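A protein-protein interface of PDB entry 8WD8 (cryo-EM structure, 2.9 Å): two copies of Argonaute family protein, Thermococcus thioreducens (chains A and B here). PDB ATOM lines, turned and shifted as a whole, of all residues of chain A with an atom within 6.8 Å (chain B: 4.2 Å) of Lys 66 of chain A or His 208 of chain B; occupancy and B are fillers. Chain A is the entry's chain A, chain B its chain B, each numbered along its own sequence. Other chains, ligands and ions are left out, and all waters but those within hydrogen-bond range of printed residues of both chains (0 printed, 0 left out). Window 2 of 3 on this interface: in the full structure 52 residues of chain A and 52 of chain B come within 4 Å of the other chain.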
ATOM      1  N   LYS A  25      17.676 -16.480  34.089  1.00  0.00           N
ATOM      2  CA  LYS A  25      17.765 -17.878  33.691  1.00  0.00           C
ATOM      3  C   LYS A  25      18.411 -17.961  32.316  1.00  0.00           C
ATOM      4  O   LYS A  25      17.921 -17.353  31.358  1.00  0.00           O
ATOM      5  CB  LYS A  25      16.382 -18.532  33.675  1.00  0.00           C
ATOM      6  CG  LYS A  25      16.414 -20.051  33.733  1.00  0.00           C
ATOM      7  CD  LYS A  25      15.138 -20.654  33.172  1.00  0.00           C
ATOM      8  CE  LYS A  25      14.592 -21.743  34.082  1.00  0.00           C
ATOM      9  NZ  LYS A  25      14.085 -21.190  35.368  1.00  0.00           N
ATOM     10  N   ILE A  26      19.503 -18.714  32.220  1.00  0.00           N
ATOM     11  CA  ILE A  26      20.313 -18.792  31.009  1.00  0.00           C
ATOM     12  C   ILE A  26      19.959 -20.072  30.264  1.00  0.00           C
ATOM     13  O   ILE A  26      19.946 -21.161  30.853  1.00  0.00           O
ATOM     14  CB  ILE A  26      21.814 -18.741  31.345  1.00  0.00           C
ATOM     15  CG1 ILE A  26      22.137 -17.473  32.137  1.00  0.00           C
ATOM     16  CG2 ILE A  26      22.660 -18.803  30.082  1.00  0.00           C
ATOM     17  CD1 ILE A  26      21.849 -16.191  31.393  1.00  0.00           C
ATOM     18  N   PHE A  27      19.669 -19.945  28.969  1.00  0.00           N
ATOM     19  CA  PHE A  27      19.267 -21.066  28.122  1.00  0.00           C
ATOM     20  C   PHE A  27      20.439 -21.446  27.221  1.00  0.00           C
ATOM     21  O   PHE A  27      20.626 -20.857  26.153  1.00  0.00           O
ATOM     22  CB  PHE A  27      18.034 -20.705  27.298  1.00  0.00           C
ATOM     23  CG  PHE A  27      16.779 -20.568  28.110  1.00  0.00           C
ATOM     24  CD1 PHE A  27      15.974 -21.669  28.358  1.00  0.00           C
ATOM     25  CD2 PHE A  27      16.400 -19.335  28.620  1.00  0.00           C
ATOM     26  CE1 PHE A  27      14.815 -21.546  29.106  1.00  0.00           C
ATOM     27  CE2 PHE A  27      15.243 -19.203  29.367  1.00  0.00           C
ATOM     28  CZ  PHE A  27      14.450 -20.310  29.610  1.00  0.00           C
ATOM     29  N   ASN A  28      21.220 -22.433  27.652  1.00  0.00           N
ATOM     30  CA  ASN A  28      22.325 -22.967  26.864  1.00  0.00           C
ATOM     31  C   ASN A  28      22.611 -24.384  27.340  1.00  0.00           C
ATOM     32  O   ASN A  28      22.232 -24.769  28.450  1.00  0.00           O
ATOM     33  CB  ASN A  28      23.579 -22.091  26.971  1.00  0.00           C
ATOM     34  CG  ASN A  28      24.271 -22.215  28.316  1.00  0.00           C
ATOM     35  OD1 ASN A  28      23.625 -22.212  29.364  1.00  0.00           O
ATOM     36  ND2 ASN A  28      25.594 -22.320  28.292  1.00  0.00           N
ATOM     37  N   TYR A  63      24.293 -10.008  28.486  1.00  0.00           N
ATOM     38  CA  TYR A  63      24.609 -11.285  27.866  1.00  0.00           C
ATOM     39  C   TYR A  63      24.215 -11.274  26.394  1.00  0.00           C
ATOM     40  O   TYR A  63      23.206 -10.681  26.004  1.00  0.00           O
ATOM     41  CB  TYR A  63      23.894 -12.425  28.595  1.00  0.00           C
ATOM     42  CG  TYR A  63      24.348 -13.808  28.186  1.00  0.00           C
ATOM     43  CD1 TYR A  63      25.699 -14.099  28.024  1.00  0.00           C
ATOM     44  CD2 TYR A  63      23.425 -14.827  27.971  1.00  0.00           C
ATOM     45  CE1 TYR A  63      26.118 -15.366  27.653  1.00  0.00           C
ATOM     46  CE2 TYR A  63      23.835 -16.096  27.600  1.00  0.00           C
ATOM     47  CZ  TYR A  63      25.181 -16.359  27.444  1.00  0.00           C
ATOM     48  OH  TYR A  63      25.591 -17.619  27.076  1.00  0.00           O
ATOM     49  N   SER A  64      25.029 -11.941  25.576  1.00  0.00           N
ATOM     50  CA  SER A  64      24.804 -11.986  24.136  1.00  0.00           C
ATOM     51  C   SER A  64      23.809 -13.067  23.733  1.00  0.00           C
ATOM     52  O   SER A  64      23.125 -12.927  22.713  1.00  0.00           O
ATOM     53  CB  SER A  64      26.130 -12.204  23.404  1.00  0.00           C
ATOM     54  OG  SER A  64      27.115 -11.288  23.847  1.00  0.00           O
ATOM     55  N   GLY A  65      23.710 -14.140  24.511  1.00  0.00           N
ATOM     56  CA  GLY A  65      22.824 -15.240  24.191  1.00  0.00           C
ATOM     57  C   GLY A  65      21.411 -15.012  24.691  1.00  0.00           C
ATOM     58  O   GLY A  65      21.005 -13.895  25.022  1.00  0.00           O
ATOM     59  N   LYS A  66      20.652 -16.102  24.745  1.00  0.00           N
ATOM     60  CA  LYS A  66      19.266 -16.059  25.185  1.00  0.00           C
ATOM     61  C   LYS A  66      19.183 -16.142  26.704  1.00  0.00           C
ATOM     62  O   LYS A  66      19.866 -16.955  27.334  1.00  0.00           O
ATOM     63  CB  LYS A  66      18.464 -17.201  24.559  1.00  0.00           C
ATOM     64  CG  LYS A  66      16.987 -16.891  24.378  1.00  0.00           C
ATOM     65  CD  LYS A  66      16.336 -17.849  23.397  1.00  0.00           C
ATOM     66  CE  LYS A  66      14.859 -17.542  23.220  1.00  0.00           C
ATOM     67  NZ  LYS A  66      14.624 -16.114  22.870  1.00  0.00           N
ATOM     68  N   PHE A  67      18.339 -15.294  27.285  1.00  0.00           N
ATOM     69  CA  PHE A  67      18.114 -15.299  28.722  1.00  0.00           C
ATOM     70  C   PHE A  67      16.682 -14.860  28.998  1.00  0.00           C
ATOM     71  O   PHE A  67      15.968 -14.395  28.107  1.00  0.00           O
ATOM     72  CB  PHE A  67      19.151 -14.427  29.457  1.00  0.00           C
ATOM     73  CG  PHE A  67      19.196 -12.984  29.005  1.00  0.00           C
ATOM     74  CD1 PHE A  67      18.358 -12.023  29.565  1.00  0.00           C
ATOM     75  CD2 PHE A  67      20.096 -12.587  28.025  1.00  0.00           C
ATOM     76  CE1 PHE A  67      18.410 -10.705  29.147  1.00  0.00           C
ATOM     77  CE2 PHE A  67      20.153 -11.270  27.603  1.00  0.00           C
ATOM     78  CZ  PHE A  67      19.310 -10.328  28.166  1.00  0.00           C
ATOM     79  N   ALA A  68      16.269 -15.016  30.254  1.00  0.00           N
ATOM     80  CA  ALA A  68      14.932 -14.637  30.684  1.00  0.00           C
ATOM     81  C   ALA A  68      15.001 -14.032  32.077  1.00  0.00           C
ATOM     82  O   ALA A  68      15.749 -14.510  32.934  1.00  0.00           O
ATOM     83  CB  ALA A  68      13.980 -15.839  30.681  1.00  0.00           C
ATOM     84  N   ILE A  69      14.217 -12.979  32.295  1.00  0.00           N
ATOM     85  CA  ILE A  69      14.172 -12.328  33.599  1.00  0.00           C
ATOM     86  C   ILE A  69      13.323 -13.173  34.538  1.00  0.00           C
ATOM     87  O   ILE A  69      12.137 -13.412  34.280  1.00  0.00           O
ATOM     88  CB  ILE A  69      13.619 -10.900  33.487  1.00  0.00           C
ATOM     89  CG1 ILE A  69      14.523 -10.031  32.606  1.00  0.00           C
ATOM     90  CG2 ILE A  69      13.458 -10.282  34.867  1.00  0.00           C
ATOM     91  CD1 ILE A  69      13.975  -9.769  31.217  1.00  0.00           C
ATOM     92  N   ASN B 204       6.388 -21.507  29.530  1.00  0.00           N
ATOM     93  CA  ASN B 204       7.266 -20.476  28.990  1.00  0.00           C
ATOM     94  C   ASN B 204       8.662 -20.991  28.675  1.00  0.00           C
ATOM     95  O   ASN B 204       9.315 -20.474  27.762  1.00  0.00           O
ATOM     96  CB  ASN B 204       7.368 -19.304  29.971  1.00  0.00           C
ATOM     97  CG  ASN B 204       6.591 -18.087  29.508  1.00  0.00           C
ATOM     98  OD1 ASN B 204       6.701 -17.669  28.355  1.00  0.00           O
ATOM     99  ND2 ASN B 204       5.800 -17.514  30.407  1.00  0.00           N
ATOM    100  N   ASP B 205       9.139 -21.997  29.413  1.00  0.00           N
ATOM    101  CA  ASP B 205      10.460 -22.552  29.140  1.00  0.00           C
ATOM    102  C   ASP B 205      10.458 -23.421  27.890  1.00  0.00           C
ATOM    103  O   ASP B 205      11.494 -23.549  27.227  1.00  0.00           O
ATOM    104  CB  ASP B 205      10.954 -23.356  30.343  1.00  0.00           C
ATOM    105  CG  ASP B 205      11.295 -22.477  31.530  1.00  0.00           C
ATOM    106  OD1 ASP B 205      11.334 -21.241  31.364  1.00  0.00           O
ATOM    107  OD2 ASP B 205      11.528 -23.024  32.628  1.00  0.00           O
ATOM    108  N   VAL B 206       9.309 -24.019  27.559  1.00  0.00           N
ATOM    109  CA  VAL B 206       9.193 -24.830  26.348  1.00  0.00           C
ATOM    110  C   VAL B 206       9.325 -23.950  25.109  1.00  0.00           C
ATOM    111  O   VAL B 206      10.039 -24.290  24.156  1.00  0.00           O
ATOM    112  CB  VAL B 206       7.864 -25.608  26.358  1.00  0.00           C
ATOM    113  CG1 VAL B 206       7.658 -26.367  25.053  1.00  0.00           C
ATOM    114  CG2 VAL B 206       7.812 -26.555  27.546  1.00  0.00           C
ATOM    115  N   GLU B 207       8.663 -22.788  25.128  1.00  0.00           N
ATOM    116  CA  GLU B 207       8.766 -21.832  24.028  1.00  0.00           C
ATOM    117  C   GLU B 207      10.175 -21.259  23.918  1.00  0.00           C
ATOM    118  O   GLU B 207      10.684 -21.054  22.810  1.00  0.00           O
ATOM    119  CB  GLU B 207       7.742 -20.712  24.222  1.00  0.00           C
ATOM    120  CG  GLU B 207       7.703 -19.678  23.105  1.00  0.00           C
ATOM    121  CD  GLU B 207       6.846 -20.113  21.935  1.00  0.00           C
ATOM    122  OE1 GLU B 207       5.613 -20.214  22.106  1.00  0.00           O
ATOM    123  OE2 GLU B 207       7.404 -20.351  20.843  1.00  0.00           O
ATOM    124  N   HIS B 208      10.829 -21.024  25.061  1.00  0.00           N
ATOM    125  CA  HIS B 208      12.194 -20.502  25.059  1.00  0.00           C
ATOM    126  C   HIS B 208      13.178 -21.519  24.490  1.00  0.00           C
ATOM    127  O   HIS B 208      14.052 -21.167  23.690  1.00  0.00           O
ATOM    128  CB  HIS B 208      12.600 -20.094  26.475  1.00  0.00           C
ATOM    129  CG  HIS B 208      12.168 -18.712  26.853  1.00  0.00           C
ATOM    130  ND1 HIS B 208      11.335 -18.459  27.922  1.00  0.00           N
ATOM    131  CD2 HIS B 208      12.457 -17.507  26.307  1.00  0.00           C
ATOM    132  CE1 HIS B 208      11.128 -17.158  28.017  1.00  0.00           C
ATOM    133  NE2 HIS B 208      11.797 -16.557  27.049  1.00  0.00           N
ATOM    134  N   TRP B 209      13.030 -22.793  24.871  1.00  0.00           N
ATOM    135  CA  TRP B 209      13.897 -23.838  24.330  1.00  0.00           C
ATOM    136  C   TRP B 209      13.627 -24.077  22.847  1.00  0.00           C
ATOM    137  O   TRP B 209      14.564 -24.327  22.077  1.00  0.00           O
ATOM    138  CB  TRP B 209      13.723 -25.135  25.122  1.00  0.00           C
ATOM    139  CG  TRP B 209      14.534 -25.207  26.389  1.00  0.00           C
ATOM    140  CD1 TRP B 209      14.053 -25.308  27.662  1.00  0.00           C
ATOM    141  CD2 TRP B 209      15.966 -25.211  26.502  1.00  0.00           C
ATOM    142  NE1 TRP B 209      15.091 -25.359  28.560  1.00  0.00           N
ATOM    143  CE2 TRP B 209      16.275 -25.304  27.874  1.00  0.00           C
ATOM    144  CE3 TRP B 209      17.015 -25.142  25.579  1.00  0.00           C
ATOM    145  CZ2 TRP B 209      17.585 -25.327  28.343  1.00  0.00           C
ATOM    146  CZ3 TRP B 209      18.316 -25.164  26.047  1.00  0.00           C
ATOM    147  CH2 TRP B 209      18.590 -25.255  27.417  1.00  0.00           C
ATOM    148  N   TYR B 210      12.359 -23.974  22.430  1.00  0.00           N
ATOM    149  CA  TYR B 210      12.001 -24.124  21.021  1.00  0.00           C
ATOM    150  C   TYR B 210      12.611 -23.013  20.173  1.00  0.00           C
ATOM    151  O   TYR B 210      13.222 -23.277  19.130  1.00  0.00           O
ATOM    152  CB  TYR B 210      10.476 -24.139  20.879  1.00  0.00           C
ATOM    153  CG  TYR B 210       9.965 -24.456  19.489  1.00  0.00           C
ATOM    154  CD1 TYR B 210       9.827 -25.772  19.065  1.00  0.00           C
ATOM    155  CD2 TYR B 210       9.603 -23.440  18.608  1.00  0.00           C
ATOM    156  CE1 TYR B 210       9.357 -26.070  17.797  1.00  0.00           C
ATOM    157  CE2 TYR B 210       9.132 -23.728  17.338  1.00  0.00           C
ATOM    158  CZ  TYR B 210       9.010 -25.045  16.940  1.00  0.00           C
ATOM    159  OH  TYR B 210       8.542 -25.337  15.680  1.00  0.00           O
ATOM    160  N   ASP B 211      12.481 -21.761  20.628  1.00  0.00           N
ATOM    161  CA  ASP B 211      13.032 -20.636  19.881  1.00  0.00           C
ATOM    162  C   ASP B 211      14.556 -20.638  19.907  1.00  0.00           C
ATOM    163  O   ASP B 211      15.194 -20.250  18.924  1.00  0.00           O
ATOM    164  CB  ASP B 211      12.486 -19.318  20.428  1.00  0.00           C
ATOM    165  CG  ASP B 211      11.076 -19.028  19.949  1.00  0.00           C
ATOM    166  OD1 ASP B 211      10.898 -18.792  18.736  1.00  0.00           O
ATOM    167  OD2 ASP B 211      10.147 -19.028  20.784  1.00  0.00           O
ATOM    168  N   TYR B 212      15.157 -21.106  21.006  1.00  0.00           N
ATOM    169  CA  TYR B 212      16.613 -21.175  21.084  1.00  0.00           C
ATOM    170  C   TYR B 212      17.169 -22.242  20.146  1.00  0.00           C
ATOM    171  O   TYR B 212      18.149 -22.000  19.429  1.00  0.00           O
ATOM    172  CB  TYR B 212      17.043 -21.436  22.527  1.00  0.00           C
ATOM    173  CG  TYR B 212      18.512 -21.738  22.689  1.00  0.00           C
ATOM    174  CD1 TYR B 212      19.475 -20.781  22.391  1.00  0.00           C
ATOM    175  CD2 TYR B 212      18.936 -22.975  23.157  1.00  0.00           C
ATOM    176  CE1 TYR B 212      20.824 -21.052  22.541  1.00  0.00           C
ATOM    177  CE2 TYR B 212      20.279 -23.254  23.315  1.00  0.00           C
ATOM    178  CZ  TYR B 212      21.218 -22.291  23.004  1.00  0.00           C
ATOM    179  OH  TYR B 212      22.556 -22.568  23.158  1.00  0.00           O
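The backbone NH (N) of Lys 25 of chain A sits at hydrogen-bond distance from the backbone carbonyl oxygen (O) of Ala 68 of chain A (3.0 Å).
N of Phe 27 of chain A sits at hydrogen-bond distance from O of Lys 66 of chain A (3.4 Å).
A ring nitrogen (ND1) of His 208 of chain B sits at hydrogen-bond distance from the backbone carbonyl oxygen (O) of Asn 204 of chain B, 2.9 Å away.
Among the printed residues, merely in contact across the chains: Lys 25 of chain A with Asp 205 of chain B, Phe 27 of chain A with Asp 205 of chain B, Phe 27 of chain A with His 208 of chain B, Phe 27 of chain A with Trp 209 of chain B, Phe 27 of chain A with Tyr 212 of chain B, Asn 28 of chain A with Trp 209 of chain B, Asn 28 of chain A with Tyr 212 of chain B, Lys 66 of chain A with His 208 of chain B and Lys 66 of chain A with Tyr 212 of chain B.
Lys 66 of chain A touches two residues of chain B.
His 208 of chain B touches just these residues of chain A: Phe 27 and Lys 66.
Printed residues of chain A within 4 Å of Asp 205 of chain B: Lys 25 and Phe 27.
Of the printed residues of chain B, Asn 28 of chain A touches Trp 209 and Tyr 212.
Printed residues of chain A within 4 Å of Trp 209 of chain B: Phe 27 (3.7 Å) and Asn 28 (3.8 Å).
Asp 211 of chain B touches none of the printed residues of chain A.
Glu 207 of chain B touches none of the printed residues of chain A.
Of the 11 printed residues of chain A, 4 touch a printed residue of chain B.
Hydrophobic or aromatic side chains of chain A that line the printed part of chain B: Phe 27.
Of the 9 printed residues of chain B, 4 touch a printed residue of chain A.
Hydrophobic or aromatic side chains of chain B within 4 Å of the printed part of chain A: His 208, Trp 209 and Tyr 212.
Along chain B the printed residues that touch a printed residue of chain A span positions 205 to 212.
Among the printed residues, 9 pairs touch across the chains.
Among the printed residues, no Asp or Glu carboxylate lies within 4 Å of a Lys or Arg side-chain nitrogen of the other chain.
No position is printed for both chains.
Of the 9 pairs that touch across the chains among the printed residues, none has its exchanged pair printed and touching as well.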
